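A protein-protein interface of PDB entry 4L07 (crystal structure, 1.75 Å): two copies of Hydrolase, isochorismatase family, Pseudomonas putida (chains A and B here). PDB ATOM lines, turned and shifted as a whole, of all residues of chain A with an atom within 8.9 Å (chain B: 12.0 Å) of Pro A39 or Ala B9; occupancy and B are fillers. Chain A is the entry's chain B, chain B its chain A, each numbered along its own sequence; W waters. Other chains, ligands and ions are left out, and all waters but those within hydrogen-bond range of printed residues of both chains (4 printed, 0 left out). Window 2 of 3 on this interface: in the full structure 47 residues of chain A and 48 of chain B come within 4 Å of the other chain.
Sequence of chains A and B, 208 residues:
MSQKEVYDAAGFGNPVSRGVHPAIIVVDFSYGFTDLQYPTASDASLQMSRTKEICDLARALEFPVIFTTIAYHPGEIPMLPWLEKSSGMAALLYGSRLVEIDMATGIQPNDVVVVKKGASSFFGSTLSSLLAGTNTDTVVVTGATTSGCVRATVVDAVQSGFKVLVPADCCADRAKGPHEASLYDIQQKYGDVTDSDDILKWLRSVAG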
ATOM      1  N   TYR A  31     -35.551 -18.954  22.557  1.00  0.00           N
ATOM      2  CA  TYR A  31     -34.256 -18.757  21.900  1.00  0.00           C
ATOM      3  C   TYR A  31     -33.731 -17.337  22.096  1.00  0.00           C
ATOM      4  O   TYR A  31     -32.527 -17.129  22.224  1.00  0.00           O
ATOM      5  CB  TYR A  31     -34.332 -19.125  20.409  1.00  0.00           C
ATOM      6  CG  TYR A  31     -34.512 -20.606  20.173  1.00  0.00           C
ATOM      7  CD1 TYR A  31     -33.534 -21.525  20.578  1.00  0.00           C
ATOM      8  CD2 TYR A  31     -35.656 -21.096  19.550  1.00  0.00           C
ATOM      9  CE1 TYR A  31     -33.692 -22.882  20.352  1.00  0.00           C
ATOM     10  CE2 TYR A  31     -35.823 -22.457  19.322  1.00  0.00           C
ATOM     11  CZ  TYR A  31     -34.842 -23.343  19.729  1.00  0.00           C
ATOM     12  OH  TYR A  31     -35.002 -24.696  19.519  1.00  0.00           O
ATOM     13  N   GLY A  32     -34.646 -16.367  22.140  1.00  0.00           N
ATOM     14  CA  GLY A  32     -34.296 -14.976  22.421  1.00  0.00           C
ATOM     15  C   GLY A  32     -33.490 -14.782  23.696  1.00  0.00           C
ATOM     16  O   GLY A  32     -32.721 -13.839  23.800  1.00  0.00           O
ATOM     17  N   PHE A  33     -33.675 -15.668  24.668  1.00  0.00           N
ATOM     18  CA  PHE A  33     -32.947 -15.581  25.936  1.00  0.00           C
ATOM     19  C   PHE A  33     -31.870 -16.649  26.128  1.00  0.00           C
ATOM     20  O   PHE A  33     -31.065 -16.547  27.059  1.00  0.00           O
ATOM     21  CB  PHE A  33     -33.928 -15.558  27.126  1.00  0.00           C
ATOM     22  CG  PHE A  33     -34.809 -14.345  27.138  1.00  0.00           C
ATOM     23  CD1 PHE A  33     -34.340 -13.132  27.644  1.00  0.00           C
ATOM     24  CD2 PHE A  33     -36.097 -14.402  26.616  1.00  0.00           C
ATOM     25  CE1 PHE A  33     -35.145 -12.000  27.633  1.00  0.00           C
ATOM     26  CE2 PHE A  33     -36.905 -13.274  26.600  1.00  0.00           C
ATOM     27  CZ  PHE A  33     -36.433 -12.074  27.105  1.00  0.00           C
ATOM     28  N   THR A  34     -31.822 -17.641  25.232  1.00  0.00           N
ATOM     29  CA  THR A  34     -30.916 -18.794  25.400  1.00  0.00           C
ATOM     30  C   THR A  34     -29.912 -18.997  24.260  1.00  0.00           C
ATOM     31  O   THR A  34     -28.956 -19.755  24.406  1.00  0.00           O
ATOM     32  CB  THR A  34     -31.697 -20.112  25.567  1.00  0.00           C
ATOM     33  OG1 THR A  34     -32.440 -20.377  24.366  1.00  0.00           O
ATOM     34  CG2 THR A  34     -32.661 -20.036  26.759  1.00  0.00           C
ATOM     35  N   ASP A  35     -30.148 -18.353  23.122  1.00  0.00           N
ATOM     36  CA  ASP A  35     -29.271 -18.522  21.964  1.00  0.00           C
ATOM     37  C   ASP A  35     -28.419 -17.272  21.814  1.00  0.00           C
ATOM     38  O   ASP A  35     -28.928 -16.197  21.496  1.00  0.00           O
ATOM     39  CB  ASP A  35     -30.112 -18.792  20.704  1.00  0.00           C
ATOM     40  CG  ASP A  35     -29.259 -19.021  19.450  1.00  0.00           C
ATOM     41  OD1 ASP A  35     -28.111 -18.538  19.396  1.00  0.00           O
ATOM     42  OD2 ASP A  35     -29.755 -19.673  18.513  1.00  0.00           O
ATOM     43  N   LEU A  36     -27.115 -17.427  22.034  1.00  0.00           N
ATOM     44  CA  LEU A  36     -26.180 -16.298  22.091  1.00  0.00           C
ATOM     45  C   LEU A  36     -25.960 -15.513  20.788  1.00  0.00           C
ATOM     46  O   LEU A  36     -25.204 -14.533  20.773  1.00  0.00           O
ATOM     47  CB  LEU A  36     -24.845 -16.736  22.708  1.00  0.00           C
ATOM     48  CG  LEU A  36     -24.874 -17.034  24.212  1.00  0.00           C
ATOM     49  CD1 LEU A  36     -23.541 -17.605  24.653  1.00  0.00           C
ATOM     50  CD2 LEU A  36     -25.203 -15.777  25.015  1.00  0.00           C
ATOM     51  N   GLN A  37     -26.625 -15.918  19.709  1.00  0.00           N
ATOM     52  CA  GLN A  37     -26.666 -15.103  18.492  1.00  0.00           C
ATOM     53  C   GLN A  37     -27.495 -13.834  18.724  1.00  0.00           C
ATOM     54  O   GLN A  37     -27.318 -12.835  18.027  1.00  0.00           O
ATOM     55  CB  GLN A  37     -27.203 -15.897  17.288  1.00  0.00           C
ATOM     56  CG  GLN A  37     -28.714 -16.099  17.282  1.00  0.00           C
ATOM     57  CD  GLN A  37     -29.223 -16.795  16.035  1.00  0.00           C
ATOM     58  OE1 GLN A  37     -29.486 -16.152  15.018  1.00  0.00           O
ATOM     59  NE2 GLN A  37     -29.393 -18.109  16.114  1.00  0.00           N
ATOM     60  N   TYR A  38     -28.393 -13.876  19.710  1.00  0.00           N
ATOM     61  CA  TYR A  38     -29.217 -12.715  20.057  1.00  0.00           C
ATOM     62  C   TYR A  38     -28.647 -11.985  21.271  1.00  0.00           C
ATOM     63  O   TYR A  38     -28.281 -12.625  22.261  1.00  0.00           O
ATOM     64  CB  TYR A  38     -30.658 -13.143  20.343  1.00  0.00           C
ATOM     65  CG  TYR A  38     -31.244 -14.050  19.292  1.00  0.00           C
ATOM     66  CD1 TYR A  38     -31.460 -13.594  17.994  1.00  0.00           C
ATOM     67  CD2 TYR A  38     -31.588 -15.365  19.602  1.00  0.00           C
ATOM     68  CE1 TYR A  38     -31.996 -14.425  17.031  1.00  0.00           C
ATOM     69  CE2 TYR A  38     -32.132 -16.203  18.643  1.00  0.00           C
ATOM     70  CZ  TYR A  38     -32.328 -15.730  17.363  1.00  0.00           C
ATOM     71  OH  TYR A  38     -32.874 -16.561  16.409  1.00  0.00           O
ATOM     72  N   PRO A  39     -28.575 -10.639  21.203  1.00  0.00           N
ATOM     73  CA  PRO A  39     -27.928  -9.873  22.277  1.00  0.00           C
ATOM     74  C   PRO A  39     -28.697  -9.898  23.605  1.00  0.00           C
ATOM     75  O   PRO A  39     -28.156  -9.491  24.630  1.00  0.00           O
ATOM     76  CB  PRO A  39     -27.847  -8.450  21.704  1.00  0.00           C
ATOM     77  CG  PRO A  39     -28.906  -8.392  20.657  1.00  0.00           C
ATOM     78  CD  PRO A  39     -29.016  -9.777  20.090  1.00  0.00           C
ATOM     79  N   THR A  40     -29.941 -10.373  23.579  1.00  0.00           N
ATOM     80  CA  THR A  40     -30.747 -10.511  24.798  1.00  0.00           C
ATOM     81  C   THR A  40     -30.465 -11.827  25.549  1.00  0.00           C
ATOM     82  O   THR A  40     -30.969 -12.048  26.658  1.00  0.00           O
ATOM     83  CB  THR A  40     -32.261 -10.420  24.492  1.00  0.00           C
ATOM     84  OG1 THR A  40     -32.569 -11.195  23.326  1.00  0.00           O
ATOM     85  CG2 THR A  40     -32.686  -8.969  24.239  1.00  0.00           C
ATOM     86  N   ALA A  41     -29.661 -12.701  24.946  1.00  0.00           N
ATOM     87  CA  ALA A  41     -29.510 -14.056  25.469  1.00  0.00           C
ATOM     88  C   ALA A  41     -28.381 -14.224  26.474  1.00  0.00           C
ATOM     89  O   ALA A  41     -27.482 -13.385  26.563  1.00  0.00           O
ATOM     90  CB  ALA A  41     -29.358 -15.054  24.320  1.00  0.00           C
ATOM     91  N   SER A  42     -28.447 -15.327  27.214  1.00  0.00           N
ATOM     92  CA  SER A  42     -27.435 -15.742  28.176  1.00  0.00           C
ATOM     93  C   SER A  42     -27.132 -17.221  27.953  1.00  0.00           C
ATOM     94  O   SER A  42     -27.935 -17.937  27.353  1.00  0.00           O
ATOM     95  CB  SER A  42     -27.969 -15.565  29.604  1.00  0.00           C
ATOM     96  OG  SER A  42     -28.412 -14.241  29.838  1.00  0.00           O
ATOM     97  N   SER A  87     -35.353  -1.782  25.468  1.00  0.00           N
ATOM     98  CA  SER A  87     -35.654  -1.720  24.033  1.00  0.00           C
ATOM     99  C   SER A  87     -35.243  -2.964  23.255  1.00  0.00           C
ATOM    100  O   SER A  87     -35.773  -3.222  22.167  1.00  0.00           O
ATOM    101  CB  SER A  87     -35.036  -0.461  23.397  1.00  0.00           C
ATOM    102  OG  SER A  87     -33.622  -0.460  23.531  1.00  0.00           O
ATOM    103  N   GLY A  88     -34.298  -3.725  23.807  1.00  0.00           N
ATOM    104  CA  GLY A  88     -33.858  -4.984  23.214  1.00  0.00           C
ATOM    105  C   GLY A  88     -34.979  -6.003  23.103  1.00  0.00           C
ATOM    106  O   GLY A  88     -34.973  -6.847  22.206  1.00  0.00           O
ATOM    107  N   MET A  89     -35.953  -5.901  24.006  1.00  0.00           N
ATOM    108  CA  MET A  89     -37.109  -6.796  24.030  1.00  0.00           C
ATOM    109  C   MET A  89     -38.029  -6.636  22.819  1.00  0.00           C
ATOM    110  O   MET A  89     -38.813  -7.533  22.522  1.00  0.00           O
ATOM    111  CB  MET A  89     -37.918  -6.609  25.325  1.00  0.00           C
ATOM    112  CG  MET A  89     -37.103  -6.806  26.598  1.00  0.00           C
ATOM    113  SD  MET A  89     -36.458  -8.483  26.747  1.00  0.00           S
ATOM    114  CE  MET A  89     -35.306  -8.275  28.102  1.00  0.00           C
ATOM    115  N   ALA A  91     -37.324  -6.897  19.853  1.00  0.00           N
ATOM    116  CA  ALA A  91     -36.946  -7.907  18.853  1.00  0.00           C
ATOM    117  C   ALA A  91     -37.777  -9.185  18.985  1.00  0.00           C
ATOM    118  O   ALA A  91     -37.801 -10.019  18.075  1.00  0.00           O
ATOM    119  CB  ALA A  91     -35.457  -8.230  18.960  1.00  0.00           C
ATOM    120  N   LEU A  92     -38.453  -9.336  20.126  1.00  0.00           N
ATOM    121  CA  LEU A  92     -39.201 -10.550  20.447  1.00  0.00           C
ATOM    122  C   LEU A  92     -40.581 -10.519  19.807  1.00  0.00           C
ATOM    123  O   LEU A  92     -41.585 -10.282  20.481  1.00  0.00           O
ATOM    124  CB  LEU A  92     -39.300 -10.730  21.969  1.00  0.00           C
ATOM    125  CG  LEU A  92     -37.963 -10.760  22.727  1.00  0.00           C
ATOM    126  CD1 LEU A  92     -38.200 -10.698  24.233  1.00  0.00           C
ATOM    127  CD2 LEU A  92     -37.154 -11.997  22.360  1.00  0.00           C
ATOM    128  N   LEU A  98     -37.019 -16.014  17.852  1.00  0.00           N
ATOM    129  CA  LEU A  98     -36.658 -15.495  19.183  1.00  0.00           C
ATOM    130  C   LEU A  98     -37.685 -15.888  20.251  1.00  0.00           C
ATOM    131  O   LEU A  98     -37.332 -16.062  21.417  1.00  0.00           O
ATOM    132  CB  LEU A  98     -36.566 -13.962  19.185  1.00  0.00           C
ATOM    133  CG  LEU A  98     -35.722 -12.990  18.329  1.00  0.00           C
ATOM    134  CD1 LEU A  98     -34.613 -12.300  19.120  1.00  0.00           C
ATOM    135  CD2 LEU A  98     -35.231 -13.555  17.004  1.00  0.00           C
ATOM    136  N   ARG A 174     -27.433 -12.904  32.934  1.00  0.00           N
ATOM    137  CA  ARG A 174     -26.377 -12.377  32.077  1.00  0.00           C
ATOM    138  C   ARG A 174     -25.218 -11.817  32.893  1.00  0.00           C
ATOM    139  O   ARG A 174     -24.198 -11.427  32.330  1.00  0.00           O
ATOM    140  CB  ARG A 174     -26.912 -11.351  31.061  1.00  0.00           C
ATOM    141  CG  ARG A 174     -28.087 -10.516  31.524  1.00  0.00           C
ATOM    142  CD  ARG A 174     -28.525  -9.509  30.470  1.00  0.00           C
ATOM    143  NE  ARG A 174     -29.565 -10.011  29.565  1.00  0.00           N
ATOM    144  CZ  ARG A 174     -30.861 -10.084  29.867  1.00  0.00           C
ATOM    145  NH1 ARG A 174     -31.297  -9.711  31.066  1.00  0.00           N
ATOM    146  NH2 ARG A 174     -31.731 -10.541  28.968  1.00  0.00           N
ATOM    147  N   MET B   1     -16.879  -9.509  26.783  1.00  0.00           N
ATOM    148  CA  MET B   1     -17.634  -8.264  27.112  1.00  0.00           C
ATOM    149  C   MET B   1     -17.800  -8.082  28.609  1.00  0.00           C
ATOM    150  O   MET B   1     -18.077  -9.041  29.330  1.00  0.00           O
ATOM    151  CB  MET B   1     -19.019  -8.285  26.469  1.00  0.00           C
ATOM    152  CG  MET B   1     -19.061  -7.836  25.020  1.00  0.00           C
ATOM    153  SD  MET B   1     -20.746  -7.917  24.387  1.00  0.00           S
ATOM    154  CE  MET B   1     -21.011  -9.689  24.353  1.00  0.00           C
ATOM    155  N   SER B   2     -17.637  -6.843  29.066  1.00  0.00           N
ATOM    156  CA  SER B   2     -17.915  -6.477  30.454  1.00  0.00           C
ATOM    157  C   SER B   2     -19.424  -6.492  30.687  1.00  0.00           C
ATOM    158  O   SER B   2     -20.205  -6.477  29.731  1.00  0.00           O
ATOM    159  CB  SER B   2     -17.375  -5.079  30.751  1.00  0.00           C
ATOM    160  OG  SER B   2     -18.139  -4.091  30.072  1.00  0.00           O
ATOM    161  N   GLN B   3     -19.832  -6.517  31.951  1.00  0.00           N
ATOM    162  CA  GLN B   3     -21.264  -6.472  32.284  1.00  0.00           C
ATOM    163  C   GLN B   3     -21.954  -5.255  31.655  1.00  0.00           C
ATOM    164  O   GLN B   3     -23.048  -5.367  31.088  1.00  0.00           O
ATOM    165  CB  GLN B   3     -21.457  -6.483  33.796  1.00  0.00           C
ATOM    166  CG  GLN B   3     -22.915  -6.423  34.234  1.00  0.00           C
ATOM    167  CD  GLN B   3     -23.072  -6.592  35.726  1.00  0.00           C
ATOM    168  OE1 GLN B   3     -22.172  -7.091  36.402  1.00  0.00           O
ATOM    169  NE2 GLN B   3     -24.219  -6.171  36.255  1.00  0.00           N
ATOM    170  N   LYS B   4     -21.302  -4.096  31.748  1.00  0.00           N
ATOM    171  CA  LYS B   4     -21.811  -2.871  31.123  1.00  0.00           C
ATOM    172  C   LYS B   4     -22.048  -3.057  29.618  1.00  0.00           C
ATOM    173  O   LYS B   4     -23.086  -2.654  29.091  1.00  0.00           O
ATOM    174  CB  LYS B   4     -20.864  -1.696  31.386  1.00  0.00           C
ATOM    175  CG  LYS B   4     -21.201  -0.428  30.614  1.00  0.00           C
ATOM    176  CD  LYS B   4     -20.168   0.663  30.874  1.00  0.00           C
ATOM    177  CE  LYS B   4     -19.799   1.398  29.594  1.00  0.00           C
ATOM    178  NZ  LYS B   4     -19.003   0.545  28.656  1.00  0.00           N
ATOM    179  N   GLU B   5     -21.084  -3.677  28.934  1.00  0.00           N
ATOM    180  CA  GLU B   5     -21.210  -3.941  27.502  1.00  0.00           C
ATOM    181  C   GLU B   5     -22.337  -4.928  27.199  1.00  0.00           C
ATOM    182  O   GLU B   5     -23.070  -4.757  26.218  1.00  0.00           O
ATOM    183  CB  GLU B   5     -19.876  -4.424  26.915  1.00  0.00           C
ATOM    184  CG  GLU B   5     -18.837  -3.312  26.828  1.00  0.00           C
ATOM    185  CD  GLU B   5     -17.403  -3.800  26.660  1.00  0.00           C
ATOM    186  OE1 GLU B   5     -17.106  -4.990  26.927  1.00  0.00           O
ATOM    187  OE2 GLU B   5     -16.558  -2.965  26.274  1.00  0.00           O
ATOM    188  N   VAL B   6     -22.479  -5.945  28.048  1.00  0.00           N
ATOM    189  CA  VAL B   6     -23.549  -6.943  27.882  1.00  0.00           C
ATOM    190  C   VAL B   6     -24.924  -6.279  27.987  1.00  0.00           C
ATOM    191  O   VAL B   6     -25.786  -6.482  27.132  1.00  0.00           O
ATOM    192  CB  VAL B   6     -23.438  -8.093  28.911  1.00  0.00           C
ATOM    193  CG1 VAL B   6     -24.702  -8.955  28.910  1.00  0.00           C
ATOM    194  CG2 VAL B   6     -22.211  -8.950  28.637  1.00  0.00           C
ATOM    195  N   TYR B   7     -25.126  -5.497  29.043  1.00  0.00           N
ATOM    196  CA  TYR B   7     -26.413  -4.821  29.258  1.00  0.00           C
ATOM    197  C   TYR B   7     -26.715  -3.793  28.160  1.00  0.00           C
ATOM    198  O   TYR B   7     -27.848  -3.705  27.672  1.00  0.00           O
ATOM    199  CB  TYR B   7     -26.463  -4.198  30.659  1.00  0.00           C
ATOM    200  CG  TYR B   7     -26.943  -5.155  31.732  1.00  0.00           C
ATOM    201  CD1 TYR B   7     -28.206  -5.006  32.313  1.00  0.00           C
ATOM    202  CD2 TYR B   7     -26.136  -6.208  32.169  1.00  0.00           C
ATOM    203  CE1 TYR B   7     -28.649  -5.885  33.293  1.00  0.00           C
ATOM    204  CE2 TYR B   7     -26.567  -7.093  33.146  1.00  0.00           C
ATOM    205  CZ  TYR B   7     -27.825  -6.924  33.705  1.00  0.00           C
ATOM    206  OH  TYR B   7     -28.247  -7.801  34.674  1.00  0.00           O
ATOM    207  N   ASP B   8     -25.691  -3.051  27.738  1.00  0.00           N
ATOM    208  CA  ASP B   8     -25.847  -2.100  26.634  1.00  0.00           C
ATOM    209  C   ASP B   8     -26.276  -2.791  25.332  1.00  0.00           C
ATOM    210  O   ASP B   8     -27.231  -2.365  24.689  1.00  0.00           O
ATOM    211  CB  ASP B   8     -24.564  -1.290  26.417  1.00  0.00           C
ATOM    212  CG  ASP B   8     -24.715  -0.245  25.322  1.00  0.00           C
ATOM    213  OD1 ASP B   8     -25.667   0.565  25.388  1.00  0.00           O
ATOM    214  OD2 ASP B   8     -23.885  -0.238  24.388  1.00  0.00           O
ATOM    215  N   ALA B   9     -25.582  -3.863  24.955  1.00  0.00           N
ATOM    216  CA  ALA B   9     -25.925  -4.583  23.730  1.00  0.00           C
ATOM    217  C   ALA B   9     -27.314  -5.225  23.806  1.00  0.00           C
ATOM    218  O   ALA B   9     -27.979  -5.373  22.780  1.00  0.00           O
ATOM    219  CB  ALA B   9     -24.869  -5.631  23.405  1.00  0.00           C
ATOM    220  N   ALA B  10     -27.740  -5.594  25.017  1.00  0.00           N
ATOM    221  CA  ALA B  10     -29.058  -6.196  25.243  1.00  0.00           C
ATOM    222  C   ALA B  10     -30.188  -5.162  25.206  1.00  0.00           C
ATOM    223  O   ALA B  10     -31.368  -5.517  25.305  1.00  0.00           O
ATOM    224  CB  ALA B  10     -29.078  -6.968  26.560  1.00  0.00           C
ATOM    225  N   GLY B  11     -29.822  -3.893  25.052  1.00  0.00           N
ATOM    226  CA  GLY B  11     -30.787  -2.811  24.872  1.00  0.00           C
ATOM    227  C   GLY B  11     -31.373  -2.261  26.161  1.00  0.00           C
ATOM    228  O   GLY B  11     -32.443  -1.648  26.145  1.00  0.00           O
ATOM    229  N   PHE B  12     -30.667  -2.458  27.274  1.00  0.00           N
ATOM    230  CA  PHE B  12     -31.112  -1.946  28.577  1.00  0.00           C
ATOM    231  C   PHE B  12     -30.583  -0.541  28.865  1.00  0.00           C
ATOM    232  O   PHE B  12     -29.679  -0.056  28.186  1.00  0.00           O
ATOM    233  CB  PHE B  12     -30.665  -2.887  29.701  1.00  0.00           C
ATOM    234  CG  PHE B  12     -31.368  -4.219  29.712  1.00  0.00           C
ATOM    235  CD1 PHE B  12     -32.745  -4.304  29.922  1.00  0.00           C
ATOM    236  CD2 PHE B  12     -30.642  -5.394  29.552  1.00  0.00           C
ATOM    237  CE1 PHE B  12     -33.384  -5.541  29.951  1.00  0.00           C
ATOM    238  CE2 PHE B  12     -31.274  -6.633  29.582  1.00  0.00           C
ATOM    239  CZ  PHE B  12     -32.648  -6.706  29.781  1.00  0.00           C
ATOM    240  N   GLY B  13     -31.154   0.103  29.880  1.00  0.00           N
ATOM    241  CA  GLY B  13     -30.614   1.352  30.413  1.00  0.00           C
ATOM    242  C   GLY B  13     -30.950   2.624  29.658  1.00  0.00           C
ATOM    243  O   GLY B  13     -30.354   3.664  29.926  1.00  0.00           O
ATOM    244  N   ASN B  14     -31.891   2.547  28.719  1.00  0.00           N
ATOM    245  CA  ASN B  14     -32.369   3.735  27.994  1.00  0.00           C
ATOM    246  C   ASN B  14     -33.094   4.713  28.916  1.00  0.00           C
ATOM    247  O   ASN B  14     -33.706   4.290  29.896  1.00  0.00           O
ATOM    248  CB  ASN B  14     -33.315   3.338  26.863  1.00  0.00           C
ATOM    249  CG  ASN B  14     -32.677   2.388  25.877  1.00  0.00           C
ATOM    250  OD1 ASN B  14     -31.892   2.799  25.028  1.00  0.00           O
ATOM    251  ND2 ASN B  14     -33.024   1.115  25.976  1.00  0.00           N
ATOM    252  N   TYR B 184     -29.976  -0.822  40.673  1.00  0.00           N
ATOM    253  CA  TYR B 184     -29.308  -1.207  39.430  1.00  0.00           C
ATOM    254  C   TYR B 184     -30.300  -1.843  38.456  1.00  0.00           C
ATOM    255  O   TYR B 184     -30.403  -1.416  37.299  1.00  0.00           O
ATOM    256  CB  TYR B 184     -28.129  -2.151  39.693  1.00  0.00           C
ATOM    257  CG  TYR B 184     -27.487  -2.649  38.410  1.00  0.00           C
ATOM    258  CD1 TYR B 184     -26.625  -1.830  37.680  1.00  0.00           C
ATOM    259  CD2 TYR B 184     -27.760  -3.928  37.916  1.00  0.00           C
ATOM    260  CE1 TYR B 184     -26.041  -2.270  36.501  1.00  0.00           C
ATOM    261  CE2 TYR B 184     -27.180  -4.379  36.736  1.00  0.00           C
ATOM    262  CZ  TYR B 184     -26.319  -3.546  36.037  1.00  0.00           C
ATOM    263  OH  TYR B 184     -25.735  -3.972  34.869  1.00  0.00           O
ATOM    264  N   GLN B 188     -31.602  -0.301  34.792  1.00  0.00           N
ATOM    265  CA  GLN B 188     -31.385  -1.063  33.572  1.00  0.00           C
ATOM    266  C   GLN B 188     -32.686  -1.414  32.853  1.00  0.00           C
ATOM    267  O   GLN B 188     -32.776  -1.267  31.630  1.00  0.00           O
ATOM    268  CB  GLN B 188     -30.575  -2.336  33.860  1.00  0.00           C
ATOM    269  CG  GLN B 188     -29.127  -2.069  34.271  1.00  0.00           C
ATOM    270  CD  GLN B 188     -28.381  -1.197  33.270  1.00  0.00           C
ATOM    271  OE1 GLN B 188     -27.655  -0.277  33.654  1.00  0.00           O
ATOM    272  NE2 GLN B 188     -28.571  -1.466  31.986  1.00  0.00           N
ATOM    273  N   LYS B 189     -33.695  -1.842  33.613  1.00  0.00           N
ATOM    274  CA  LYS B 189     -34.848  -2.535  33.018  1.00  0.00           C
ATOM    275  C   LYS B 189     -36.212  -1.872  33.166  1.00  0.00           C
ATOM    276  O   LYS B 189     -37.106  -2.119  32.350  1.00  0.00           O
ATOM    277  CB  LYS B 189     -34.950  -3.965  33.564  1.00  0.00           C
ATOM    278  CG  LYS B 189     -33.686  -4.794  33.393  1.00  0.00           C
ATOM    279  CD  LYS B 189     -33.923  -6.246  33.786  1.00  0.00           C
ATOM    280  CE  LYS B 189     -32.633  -7.055  33.706  1.00  0.00           C
ATOM    281  NZ  LYS B 189     -32.816  -8.445  34.210  1.00  0.00           N
HETATM  282  O   HOH W   1     -30.224  -9.505  33.756  1.00  0.00           O
HETATM  283  O   HOH W   2     -33.690  -4.867  26.629  1.00  0.00           O
HETATM  284  O   HOH W   3     -30.481   0.839  23.509  1.00  0.00           O
HETATM  285  O   HOH W   4     -25.645  -8.467  25.212  1.00  0.00           O
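CB of Pro A39 touches O of Ala B9, at 3.3 Å.
Pro A39 touches Ala B10.
Ala B10 touches Thr A40 (O to CG2, 3.8 Å).
Ala B10 touches Gly A88 (O to CA, 3.3 Å).
Gly B11 touches Gly A88 (O to N, 3.6 Å).
Met A89 touches Phe B12.
Arg A174 touches Val B6 (CB to CG1, 3.9 Å).
Phe B12 touches Arg A174 (CE2 to NH1, 3.4 Å).
Arg A174 touches Lys B189 (NH1 to NZ, 3.7 Å).
Of the printed residues of chain B, Pro A39 touches Ala B9 and Ala B10.
Printed residues of chain B within 4 Å of Thr A40: Ala B10 (3.8 Å).
No residue of chain B comes within 4 Å of Ala A41.
Of the printed residues of chain B, Ser A87 touches Gly B11 and Asn B14.
Of chain B, only Ala B10 (3.3 Å) and Gly B11 (3.6 Å) come within 4 Å of Gly A88.
Of the printed residues of chain B, Met A89 touches Phe B12 (3.5 Å).
Tyr B7 touches none of the printed residues of chain A.
No residue of chain A comes within 4 Å of Asp B8.
Ala B9 touches one residue of chain A.
Ala B10 touches just these residues of chain A: Pro A39, Thr A40 and Gly A88.
Printed residues of chain A within 4 Å of Gly B11: Ser A87 and Gly A88.
Of the printed residues of chain A, Asn B14 touches Ser A87.
Of the printed residues of chain A, Lys B189 touches Arg A174 (3.7 Å).
The nearest residue of chain B that does not touch Pro A39 is Val B6 (4.6 Å).
The nearest residue of chain A that does not touch Ala B9 is Thr A40 (5.4 Å).
The backbone NH of Phe B12 is in hydrogen-bond range of the backbone carbonyl oxygen of Tyr B7, at 3.1 Å.
The backbone carbonyl oxygen (O) of Gly B11 is in hydrogen-bond range of the side-chain amide nitrogen (ND2) of Asn B14 (2.8 Å).
The backbone carbonyl oxygen (O) of Gly A32 lies within hydrogen-bond range of the side-chain hydroxyl (OG1) of Thr A40.
NH2 of Arg A174 lies within hydrogen-bond range of O of Thr A40, at 2.9 Å.
Hydrophobic or aromatic side chains of chain A within 4 Å of the printed part of chain B: Pro A39 and Met A89.
Of the 17 printed residues of chain B, 7 touch a printed residue of chain A.
Printed residues of chain B that touch a printed residue of chain A: Val B6, Ala B9, Ala B10, Gly B11, Phe B12, Asn B14 and Lys B189.
Along chain B the printed residues that touch a printed residue of chain A span positions 6 to 189.
Among the printed residues, 11 pairs touch across the chains.
Among the printed residues, no Asp or Glu carboxylate lies within 4 Å of a Lys or Arg side-chain nitrogen of the other chain.
No position is printed for both chains.
Of the 11 pairs that touch across the chains among the printed residues, none has its exchanged pair printed and touching as well.
The backbone carbonyl oxygen (O) of Gly B11 is in hydrogen-bond range of the backbone NH (N) of Ser A87, at 3.0 Å.
ND2 of Asn B14 is in hydrogen-bond range of OG of Ser A87, 3.0 Å away.
Water W2 lies within hydrogen-bond range of the backbone carbonyl oxygen of Ala B10 (2.8 Å), the backbone NH of Gly A88 (3.1 Å) and the backbone carbonyl oxygen of Gly B11 (3.5 Å).
Water W4 lies within hydrogen-bond range of the backbone carbonyl oxygen of Val B6 and the backbone carbonyl oxygen of Pro A39.
Water W1 lies within hydrogen-bond range of the side-chain hydroxyl (OH) of Tyr B7 (2.8 Å), the side-chain amino group (NZ) of Lys B189 (2.8 Å) and the guanidinium group (NH1) of Arg A174 (2.9 Å).
Water W3 bridges OD1 of Asn B14 (2.9 Å) and OG of Ser A87 (3.4 Å).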
